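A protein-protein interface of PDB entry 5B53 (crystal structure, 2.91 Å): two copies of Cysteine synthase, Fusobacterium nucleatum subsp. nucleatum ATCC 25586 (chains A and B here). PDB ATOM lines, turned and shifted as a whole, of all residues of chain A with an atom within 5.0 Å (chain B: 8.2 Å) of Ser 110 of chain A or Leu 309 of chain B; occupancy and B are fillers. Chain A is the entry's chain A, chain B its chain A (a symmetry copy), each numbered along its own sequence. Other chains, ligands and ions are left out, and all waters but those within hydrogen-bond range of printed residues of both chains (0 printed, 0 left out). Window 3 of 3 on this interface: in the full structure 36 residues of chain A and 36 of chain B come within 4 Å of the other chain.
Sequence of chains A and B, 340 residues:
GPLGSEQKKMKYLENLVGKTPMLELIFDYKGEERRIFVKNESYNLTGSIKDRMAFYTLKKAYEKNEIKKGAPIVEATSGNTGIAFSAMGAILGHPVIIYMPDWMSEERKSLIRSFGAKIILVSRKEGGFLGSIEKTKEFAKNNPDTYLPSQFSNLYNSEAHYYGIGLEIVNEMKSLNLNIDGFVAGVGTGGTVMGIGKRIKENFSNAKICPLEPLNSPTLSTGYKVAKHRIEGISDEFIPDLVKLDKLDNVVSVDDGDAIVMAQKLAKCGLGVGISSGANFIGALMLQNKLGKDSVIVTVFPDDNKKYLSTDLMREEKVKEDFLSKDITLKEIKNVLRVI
2 positions are printed for both chains. Of the 7 pairs that touch across the chains among the printed residues, none has its exchanged pair printed and touching as well.
Among the printed residues, pairs that only touch across the chains: Glu 107 of chain A with Leu 309 of chain B (3.9 Å), Ser 110 of chain A with Leu 309 of chain B (3.9 Å), Ser 110 of chain A with Met 314 of chain B (3.3 Å), Leu 111 of chain A with Asn 305 of chain B (3.7 Å), Ser 114 of chain A with Ala 267 of chain B (3.1 Å) and Ser 114 of chain A with Met 314 of chain B (3.8 Å).
OG of Ser 114 of chain A is in hydrogen-bond range of OD1 of Asn 305 of chain B.
Lys 109 of chain A touches none of the printed residues of chain B. Printed residues of chain B within 4 Å of Leu 111 of chain A: Asn 305. Printed residues of chain A within 4 Å of Ala 267 of chain B: Ser 114 (3.1 Å). Leu 309 of chain B touches two residues of chain A.
The backbone carbonyl oxygen of Leu 111 of chain A is in hydrogen-bond range of the side-chain hydroxyl of Ser 114 of chain A, at 2.9 Å.
Among the printed residues, 7 pairs touch across the chains. Among the printed residues, no Asp or Glu carboxylate lies within 4 Å of a Lys or Arg side-chain nitrogen of the other chain.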
ATOM      1  N   GLU A 106      24.433  31.113 -28.040  1.00  0.00           N
ATOM      2  CA  GLU A 106      25.009  29.823 -28.408  1.00  0.00           C
ATOM      3  C   GLU A 106      24.985  28.898 -27.195  1.00  0.00           C
ATOM      4  O   GLU A 106      24.783  27.703 -27.334  1.00  0.00           O
ATOM      5  CB  GLU A 106      26.431  30.010 -28.953  1.00  0.00           C
ATOM      6  CG  GLU A 106      26.530  29.850 -30.451  1.00  0.00           C
ATOM      7  CD  GLU A 106      26.653  28.375 -30.836  1.00  0.00           C
ATOM      8  OE1 GLU A 106      27.641  27.712 -30.394  1.00  0.00           O
ATOM      9  OE2 GLU A 106      25.759  27.878 -31.582  1.00  0.00           O
ATOM     10  N   GLU A 107      25.184  29.489 -26.018  1.00  0.00           N
ATOM     11  CA  GLU A 107      25.130  28.806 -24.714  1.00  0.00           C
ATOM     12  C   GLU A 107      23.872  27.919 -24.607  1.00  0.00           C
ATOM     13  O   GLU A 107      23.989  26.705 -24.430  1.00  0.00           O
ATOM     14  CB  GLU A 107      25.168  29.894 -23.592  1.00  0.00           C
ATOM     15  CG  GLU A 107      25.398  29.491 -22.124  1.00  0.00           C
ATOM     16  CD  GLU A 107      25.531  30.732 -21.240  1.00  0.00           C
ATOM     17  OE1 GLU A 107      25.209  31.804 -21.798  1.00  0.00           O
ATOM     18  OE2 GLU A 107      25.952  30.667 -20.031  1.00  0.00           O
ATOM     19  N   ARG A 108      22.694  28.528 -24.749  1.00  0.00           N
ATOM     20  CA  ARG A 108      21.430  27.802 -24.649  1.00  0.00           C
ATOM     21  C   ARG A 108      21.327  26.673 -25.658  1.00  0.00           C
ATOM     22  O   ARG A 108      20.826  25.586 -25.351  1.00  0.00           O
ATOM     23  CB  ARG A 108      20.214  28.668 -24.994  1.00  0.00           C
ATOM     24  CG  ARG A 108      20.264  30.168 -24.712  1.00  0.00           C
ATOM     25  CD  ARG A 108      20.333  30.480 -23.232  1.00  0.00           C
ATOM     26  NE  ARG A 108      19.508  29.555 -22.451  1.00  0.00           N
ATOM     27  CZ  ARG A 108      19.647  29.351 -21.149  1.00  0.00           C
ATOM     28  NH1 ARG A 108      20.582  29.981 -20.412  1.00  0.00           N
ATOM     29  NH2 ARG A 108      18.831  28.489 -20.590  1.00  0.00           N
ATOM     30  N   LYS A 109      21.735  26.978 -26.885  1.00  0.00           N
ATOM     31  CA  LYS A 109      21.368  26.158 -28.024  1.00  0.00           C
ATOM     32  C   LYS A 109      22.083  24.876 -27.861  1.00  0.00           C
ATOM     33  O   LYS A 109      21.503  23.813 -28.023  1.00  0.00           O
ATOM     34  CB  LYS A 109      21.723  26.840 -29.354  1.00  0.00           C
ATOM     35  CG  LYS A 109      20.845  28.073 -29.631  1.00  0.00           C
ATOM     36  CD  LYS A 109      20.965  28.585 -31.055  1.00  0.00           C
ATOM     37  CE  LYS A 109      22.139  29.536 -31.288  1.00  0.00           C
ATOM     38  NZ  LYS A 109      22.231  29.811 -32.754  1.00  0.00           N
ATOM     39  N   SER A 110      23.355  25.034 -27.520  1.00  0.00           N
ATOM     40  CA  SER A 110      24.303  23.997 -27.144  1.00  0.00           C
ATOM     41  C   SER A 110      23.783  22.982 -26.137  1.00  0.00           C
ATOM     42  O   SER A 110      23.954  21.776 -26.267  1.00  0.00           O
ATOM     43  CB  SER A 110      25.483  24.714 -26.498  1.00  0.00           C
ATOM     44  OG  SER A 110      26.661  24.111 -26.922  1.00  0.00           O
ATOM     45  N   LEU A 111      23.180  23.506 -25.090  1.00  0.00           N
ATOM     46  CA  LEU A 111      22.676  22.659 -24.059  1.00  0.00           C
ATOM     47  C   LEU A 111      21.502  21.856 -24.641  1.00  0.00           C
ATOM     48  O   LEU A 111      21.490  20.628 -24.606  1.00  0.00           O
ATOM     49  CB  LEU A 111      22.260  23.488 -22.834  1.00  0.00           C
ATOM     50  CG  LEU A 111      22.019  22.763 -21.497  1.00  0.00           C
ATOM     51  CD1 LEU A 111      23.105  21.737 -21.169  1.00  0.00           C
ATOM     52  CD2 LEU A 111      21.965  23.758 -20.367  1.00  0.00           C
ATOM     53  N   ILE A 112      20.533  22.522 -25.220  1.00  0.00           N
ATOM     54  CA  ILE A 112      19.393  21.806 -25.637  1.00  0.00           C
ATOM     55  C   ILE A 112      19.862  20.751 -26.611  1.00  0.00           C
ATOM     56  O   ILE A 112      19.517  19.571 -26.507  1.00  0.00           O
ATOM     57  CB  ILE A 112      18.346  22.778 -26.207  1.00  0.00           C
ATOM     58  CG1 ILE A 112      17.523  23.397 -25.041  1.00  0.00           C
ATOM     59  CG2 ILE A 112      17.397  22.090 -27.215  1.00  0.00           C
ATOM     60  CD1 ILE A 112      17.112  24.832 -25.265  1.00  0.00           C
ATOM     61  N   ARG A 113      20.669  21.186 -27.557  1.00  0.00           N
ATOM     62  CA  ARG A 113      21.240  20.288 -28.535  1.00  0.00           C
ATOM     63  C   ARG A 113      21.951  19.101 -27.954  1.00  0.00           C
ATOM     64  O   ARG A 113      21.860  18.034 -28.539  1.00  0.00           O
ATOM     65  CB  ARG A 113      22.254  20.984 -29.419  1.00  0.00           C
ATOM     66  CG  ARG A 113      21.733  21.276 -30.780  1.00  0.00           C
ATOM     67  CD  ARG A 113      22.848  21.777 -31.710  1.00  0.00           C
ATOM     68  NE  ARG A 113      23.105  23.215 -31.558  1.00  0.00           N
ATOM     69  CZ  ARG A 113      24.269  23.720 -31.224  1.00  0.00           C
ATOM     70  NH1 ARG A 113      25.317  22.938 -31.034  1.00  0.00           N
ATOM     71  NH2 ARG A 113      24.378  25.023 -31.077  1.00  0.00           N
ATOM     72  N   SER A 114      22.678  19.280 -26.851  1.00  0.00           N
ATOM     73  CA  SER A 114      23.508  18.183 -26.272  1.00  0.00           C
ATOM     74  C   SER A 114      22.713  16.909 -25.994  1.00  0.00           C
ATOM     75  O   SER A 114      23.288  15.797 -26.044  1.00  0.00           O
ATOM     76  CB  SER A 114      24.270  18.596 -24.982  1.00  0.00           C
ATOM     77  OG  SER A 114      23.419  18.625 -23.866  1.00  0.00           O
ATOM     78  N   GLU B 107      34.586  31.720 -17.500  1.00  0.00           N
ATOM     79  CA  GLU B 107      33.516  30.775 -17.137  1.00  0.00           C
ATOM     80  C   GLU B 107      33.754  30.185 -15.731  1.00  0.00           C
ATOM     81  O   GLU B 107      32.918  30.358 -14.842  1.00  0.00           O
ATOM     82  CB  GLU B 107      33.459  29.660 -18.230  1.00  0.00           C
ATOM     83  CG  GLU B 107      32.273  28.678 -18.282  1.00  0.00           C
ATOM     84  CD  GLU B 107      32.374  27.776 -19.512  1.00  0.00           C
ATOM     85  OE1 GLU B 107      33.473  27.829 -20.106  1.00  0.00           O
ATOM     86  OE2 GLU B 107      31.400  27.040 -19.901  1.00  0.00           O
ATOM     87  N   ARG B 108      34.899  29.529 -15.541  1.00  0.00           N
ATOM     88  CA  ARG B 108      35.233  28.908 -14.261  1.00  0.00           C
ATOM     89  C   ARG B 108      35.245  29.905 -13.117  1.00  0.00           C
ATOM     90  O   ARG B 108      34.790  29.608 -12.007  1.00  0.00           O
ATOM     91  CB  ARG B 108      36.656  28.342 -14.224  1.00  0.00           C
ATOM     92  CG  ARG B 108      37.288  27.828 -15.516  1.00  0.00           C
ATOM     93  CD  ARG B 108      36.586  26.601 -16.059  1.00  0.00           C
ATOM     94  NE  ARG B 108      36.157  25.709 -14.980  1.00  0.00           N
ATOM     95  CZ  ARG B 108      35.230  24.772 -15.113  1.00  0.00           C
ATOM     96  NH1 ARG B 108      34.580  24.554 -16.272  1.00  0.00           N
ATOM     97  NH2 ARG B 108      34.953  24.052 -14.051  1.00  0.00           N
ATOM     98  N   GLU B 232      38.800  16.788 -17.813  1.00  0.00           N
ATOM     99  CA  GLU B 232      38.831  17.620 -16.590  1.00  0.00           C
ATOM    100  C   GLU B 232      38.336  16.941 -15.337  1.00  0.00           C
ATOM    101  O   GLU B 232      37.185  16.431 -15.331  1.00  0.00           O
ATOM    102  CB  GLU B 232      37.843  18.753 -16.682  1.00  0.00           C
ATOM    103  CG  GLU B 232      38.298  19.887 -17.530  1.00  0.00           C
ATOM    104  CD  GLU B 232      37.576  21.172 -17.182  1.00  0.00           C
ATOM    105  OE1 GLU B 232      37.384  21.493 -15.969  1.00  0.00           O
ATOM    106  OE2 GLU B 232      37.209  21.834 -18.181  1.00  0.00           O
ATOM    107  N   ALA B 267      24.683  11.960 -23.189  1.00  0.00           N
ATOM    108  CA  ALA B 267      23.767  13.095 -23.252  1.00  0.00           C
ATOM    109  C   ALA B 267      22.611  12.892 -24.255  1.00  0.00           C
ATOM    110  O   ALA B 267      21.425  13.231 -23.976  1.00  0.00           O
ATOM    111  CB  ALA B 267      24.530  14.349 -23.577  1.00  0.00           C
ATOM    112  N   ILE B 275      33.092  15.185 -19.204  1.00  0.00           N
ATOM    113  CA  ILE B 275      33.975  14.346 -19.992  1.00  0.00           C
ATOM    114  C   ILE B 275      34.509  13.222 -19.151  1.00  0.00           C
ATOM    115  O   ILE B 275      34.500  12.083 -19.568  1.00  0.00           O
ATOM    116  CB  ILE B 275      35.139  15.154 -20.561  1.00  0.00           C
ATOM    117  CG1 ILE B 275      34.616  16.385 -21.329  1.00  0.00           C
ATOM    118  CG2 ILE B 275      35.965  14.268 -21.463  1.00  0.00           C
ATOM    119  CD1 ILE B 275      35.727  17.312 -21.793  1.00  0.00           C
ATOM    120  N   ASP B 304      27.885  16.995 -14.385  1.00  0.00           N
ATOM    121  CA  ASP B 304      27.022  17.113 -15.535  1.00  0.00           C
ATOM    122  C   ASP B 304      27.766  17.949 -16.584  1.00  0.00           C
ATOM    123  O   ASP B 304      28.802  18.512 -16.317  1.00  0.00           O
ATOM    124  CB  ASP B 304      25.631  17.675 -15.106  1.00  0.00           C
ATOM    125  CG  ASP B 304      25.608  19.192 -14.994  1.00  0.00           C
ATOM    126  OD1 ASP B 304      26.371  19.810 -15.742  1.00  0.00           O
ATOM    127  OD2 ASP B 304      24.856  19.793 -14.199  1.00  0.00           O
ATOM    128  N   ASN B 305      27.226  17.989 -17.783  1.00  0.00           N
ATOM    129  CA  ASN B 305      27.717  18.808 -18.900  1.00  0.00           C
ATOM    130  C   ASN B 305      27.591  20.359 -18.861  1.00  0.00           C
ATOM    131  O   ASN B 305      28.199  21.015 -19.665  1.00  0.00           O
ATOM    132  CB  ASN B 305      27.032  18.301 -20.179  1.00  0.00           C
ATOM    133  CG  ASN B 305      25.518  18.631 -20.254  1.00  0.00           C
ATOM    134  OD1 ASN B 305      24.927  18.506 -21.323  1.00  0.00           O
ATOM    135  ND2 ASN B 305      24.902  19.080 -19.154  1.00  0.00           N
ATOM    136  N   LYS B 306      26.835  20.957 -17.968  1.00  0.00           N
ATOM    137  CA  LYS B 306      26.595  22.402 -18.049  1.00  0.00           C
ATOM    138  C   LYS B 306      27.846  23.262 -18.010  1.00  0.00           C
ATOM    139  O   LYS B 306      27.869  24.341 -18.683  1.00  0.00           O
ATOM    140  CB  LYS B 306      25.689  22.910 -16.920  1.00  0.00           C
ATOM    141  CG  LYS B 306      24.219  22.491 -17.022  1.00  0.00           C
ATOM    142  CD  LYS B 306      23.263  23.354 -16.178  1.00  0.00           C
ATOM    143  CE  LYS B 306      22.295  22.537 -15.360  1.00  0.00           C
ATOM    144  NZ  LYS B 306      21.847  21.358 -16.124  1.00  0.00           N
ATOM    145  N   LYS B 307      28.858  22.846 -17.223  1.00  0.00           N
ATOM    146  CA  LYS B 307      30.161  23.577 -17.216  1.00  0.00           C
ATOM    147  C   LYS B 307      31.046  23.405 -18.471  1.00  0.00           C
ATOM    148  O   LYS B 307      31.892  24.231 -18.722  1.00  0.00           O
ATOM    149  CB  LYS B 307      30.998  23.224 -15.989  1.00  0.00           C
ATOM    150  CG  LYS B 307      30.511  23.859 -14.672  1.00  0.00           C
ATOM    151  CD  LYS B 307      31.370  23.481 -13.459  1.00  0.00           C
ATOM    152  CE  LYS B 307      31.771  22.020 -13.443  1.00  0.00           C
ATOM    153  NZ  LYS B 307      30.609  21.070 -13.596  1.00  0.00           N
ATOM    154  N   TYR B 308      30.801  22.384 -19.272  1.00  0.00           N
ATOM    155  CA  TYR B 308      31.702  21.968 -20.316  1.00  0.00           C
ATOM    156  C   TYR B 308      31.231  22.445 -21.677  1.00  0.00           C
ATOM    157  O   TYR B 308      31.420  21.830 -22.721  1.00  0.00           O
ATOM    158  CB  TYR B 308      31.726  20.457 -20.277  1.00  0.00           C
ATOM    159  CG  TYR B 308      32.248  19.954 -18.960  1.00  0.00           C
ATOM    160  CD1 TYR B 308      31.412  19.757 -17.904  1.00  0.00           C
ATOM    161  CD2 TYR B 308      33.596  19.734 -18.771  1.00  0.00           C
ATOM    162  CE1 TYR B 308      31.886  19.342 -16.686  1.00  0.00           C
ATOM    163  CE2 TYR B 308      34.080  19.294 -17.555  1.00  0.00           C
ATOM    164  CZ  TYR B 308      33.206  19.106 -16.507  1.00  0.00           C
ATOM    165  OH  TYR B 308      33.629  18.641 -15.293  1.00  0.00           O
ATOM    166  N   LEU B 309      30.628  23.604 -21.663  1.00  0.00           N
ATOM    167  CA  LEU B 309      29.730  23.954 -22.734  1.00  0.00           C
ATOM    168  C   LEU B 309      30.453  24.679 -23.829  1.00  0.00           C
ATOM    169  O   LEU B 309      29.907  24.853 -24.889  1.00  0.00           O
ATOM    170  CB  LEU B 309      28.585  24.795 -22.165  1.00  0.00           C
ATOM    171  CG  LEU B 309      27.210  24.407 -22.696  1.00  0.00           C
ATOM    172  CD1 LEU B 309      27.016  22.907 -22.921  1.00  0.00           C
ATOM    173  CD2 LEU B 309      26.154  24.919 -21.747  1.00  0.00           C
ATOM    174  N   SER B 310      31.678  25.124 -23.566  1.00  0.00           N
ATOM    175  CA  SER B 310      32.555  25.643 -24.599  1.00  0.00           C
ATOM    176  C   SER B 310      33.865  24.837 -24.560  1.00  0.00           C
ATOM    177  O   SER B 310      34.955  25.402 -24.600  1.00  0.00           O
ATOM    178  CB  SER B 310      32.841  27.055 -24.247  1.00  0.00           C
ATOM    179  OG  SER B 310      33.491  26.993 -23.014  1.00  0.00           O
ATOM    180  N   THR B 311      33.728  23.521 -24.415  1.00  0.00           N
ATOM    181  CA  THR B 311      34.827  22.598 -24.450  1.00  0.00           C
ATOM    182  C   THR B 311      34.591  21.658 -25.591  1.00  0.00           C
ATOM    183  O   THR B 311      33.503  21.644 -26.169  1.00  0.00           O
ATOM    184  CB  THR B 311      34.920  21.678 -23.209  1.00  0.00           C
ATOM    185  OG1 THR B 311      33.871  20.694 -23.225  1.00  0.00           O
ATOM    186  CG2 THR B 311      34.874  22.449 -21.953  1.00  0.00           C
ATOM    187  N   ASP B 312      35.580  20.793 -25.834  1.00  0.00           N
ATOM    188  CA  ASP B 312      35.547  19.932 -27.001  1.00  0.00           C
ATOM    189  C   ASP B 312      34.400  18.962 -26.961  1.00  0.00           C
ATOM    190  O   ASP B 312      34.129  18.284 -27.981  1.00  0.00           O
ATOM    191  CB  ASP B 312      36.879  19.214 -27.247  1.00  0.00           C
ATOM    192  CG  ASP B 312      37.895  20.081 -28.031  1.00  0.00           C
ATOM    193  OD1 ASP B 312      37.535  21.219 -28.474  1.00  0.00           O
ATOM    194  OD2 ASP B 312      39.071  19.614 -28.160  1.00  0.00           O
ATOM    195  N   LEU B 313      33.692  18.958 -25.824  1.00  0.00           N
ATOM    196  CA  LEU B 313      32.443  18.229 -25.684  1.00  0.00           C
ATOM    197  C   LEU B 313      31.363  18.689 -26.635  1.00  0.00           C
ATOM    198  O   LEU B 313      30.506  17.880 -26.979  1.00  0.00           O
ATOM    199  CB  LEU B 313      31.909  18.310 -24.242  1.00  0.00           C
ATOM    200  CG  LEU B 313      30.728  17.374 -23.836  1.00  0.00           C
ATOM    201  CD1 LEU B 313      31.067  15.888 -23.916  1.00  0.00           C
ATOM    202  CD2 LEU B 313      30.246  17.672 -22.434  1.00  0.00           C
ATOM    203  N   MET B 314      31.370  19.954 -27.070  1.00  0.00           N
ATOM    204  CA  MET B 314      30.332  20.428 -28.022  1.00  0.00           C
ATOM    205  C   MET B 314      30.810  20.538 -29.480  1.00  0.00           C
ATOM    206  O   MET B 314      30.243  21.293 -30.266  1.00  0.00           O
ATOM    207  CB  MET B 314      29.745  21.748 -27.547  1.00  0.00           C
ATOM    208  CG  MET B 314      29.300  21.735 -26.076  1.00  0.00           C
ATOM    209  SD  MET B 314      28.021  20.546 -25.550  1.00  0.00           S
ATOM    210  CE  MET B 314      26.888  20.529 -27.014  1.00  0.00           C
ATOM    211  N   ARG B 315      31.818  19.729 -29.826  1.00  0.00           N
ATOM    212  CA  ARG B 315      32.482  19.705 -31.125  1.00  0.00           C
ATOM    213  C   ARG B 315      32.670  18.302 -31.576  1.00  0.00           C
ATOM    214  O   ARG B 315      32.966  17.440 -30.773  1.00  0.00           O
ATOM    215  CB  ARG B 315      33.881  20.364 -31.042  1.00  0.00           C
ATOM    216  CG  ARG B 315      33.799  21.889 -30.945  1.00  0.00           C
ATOM    217  CD  ARG B 315      35.100  22.627 -30.695  1.00  0.00           C
ATOM    218  NE  ARG B 315      35.159  23.100 -29.311  1.00  0.00           N
ATOM    219  CZ  ARG B 315      35.346  24.360 -28.890  1.00  0.00           C
ATOM    220  NH1 ARG B 315      35.515  25.376 -29.729  1.00  0.00           N
ATOM    221  NH2 ARG B 315      35.375  24.610 -27.583  1.00  0.00           N
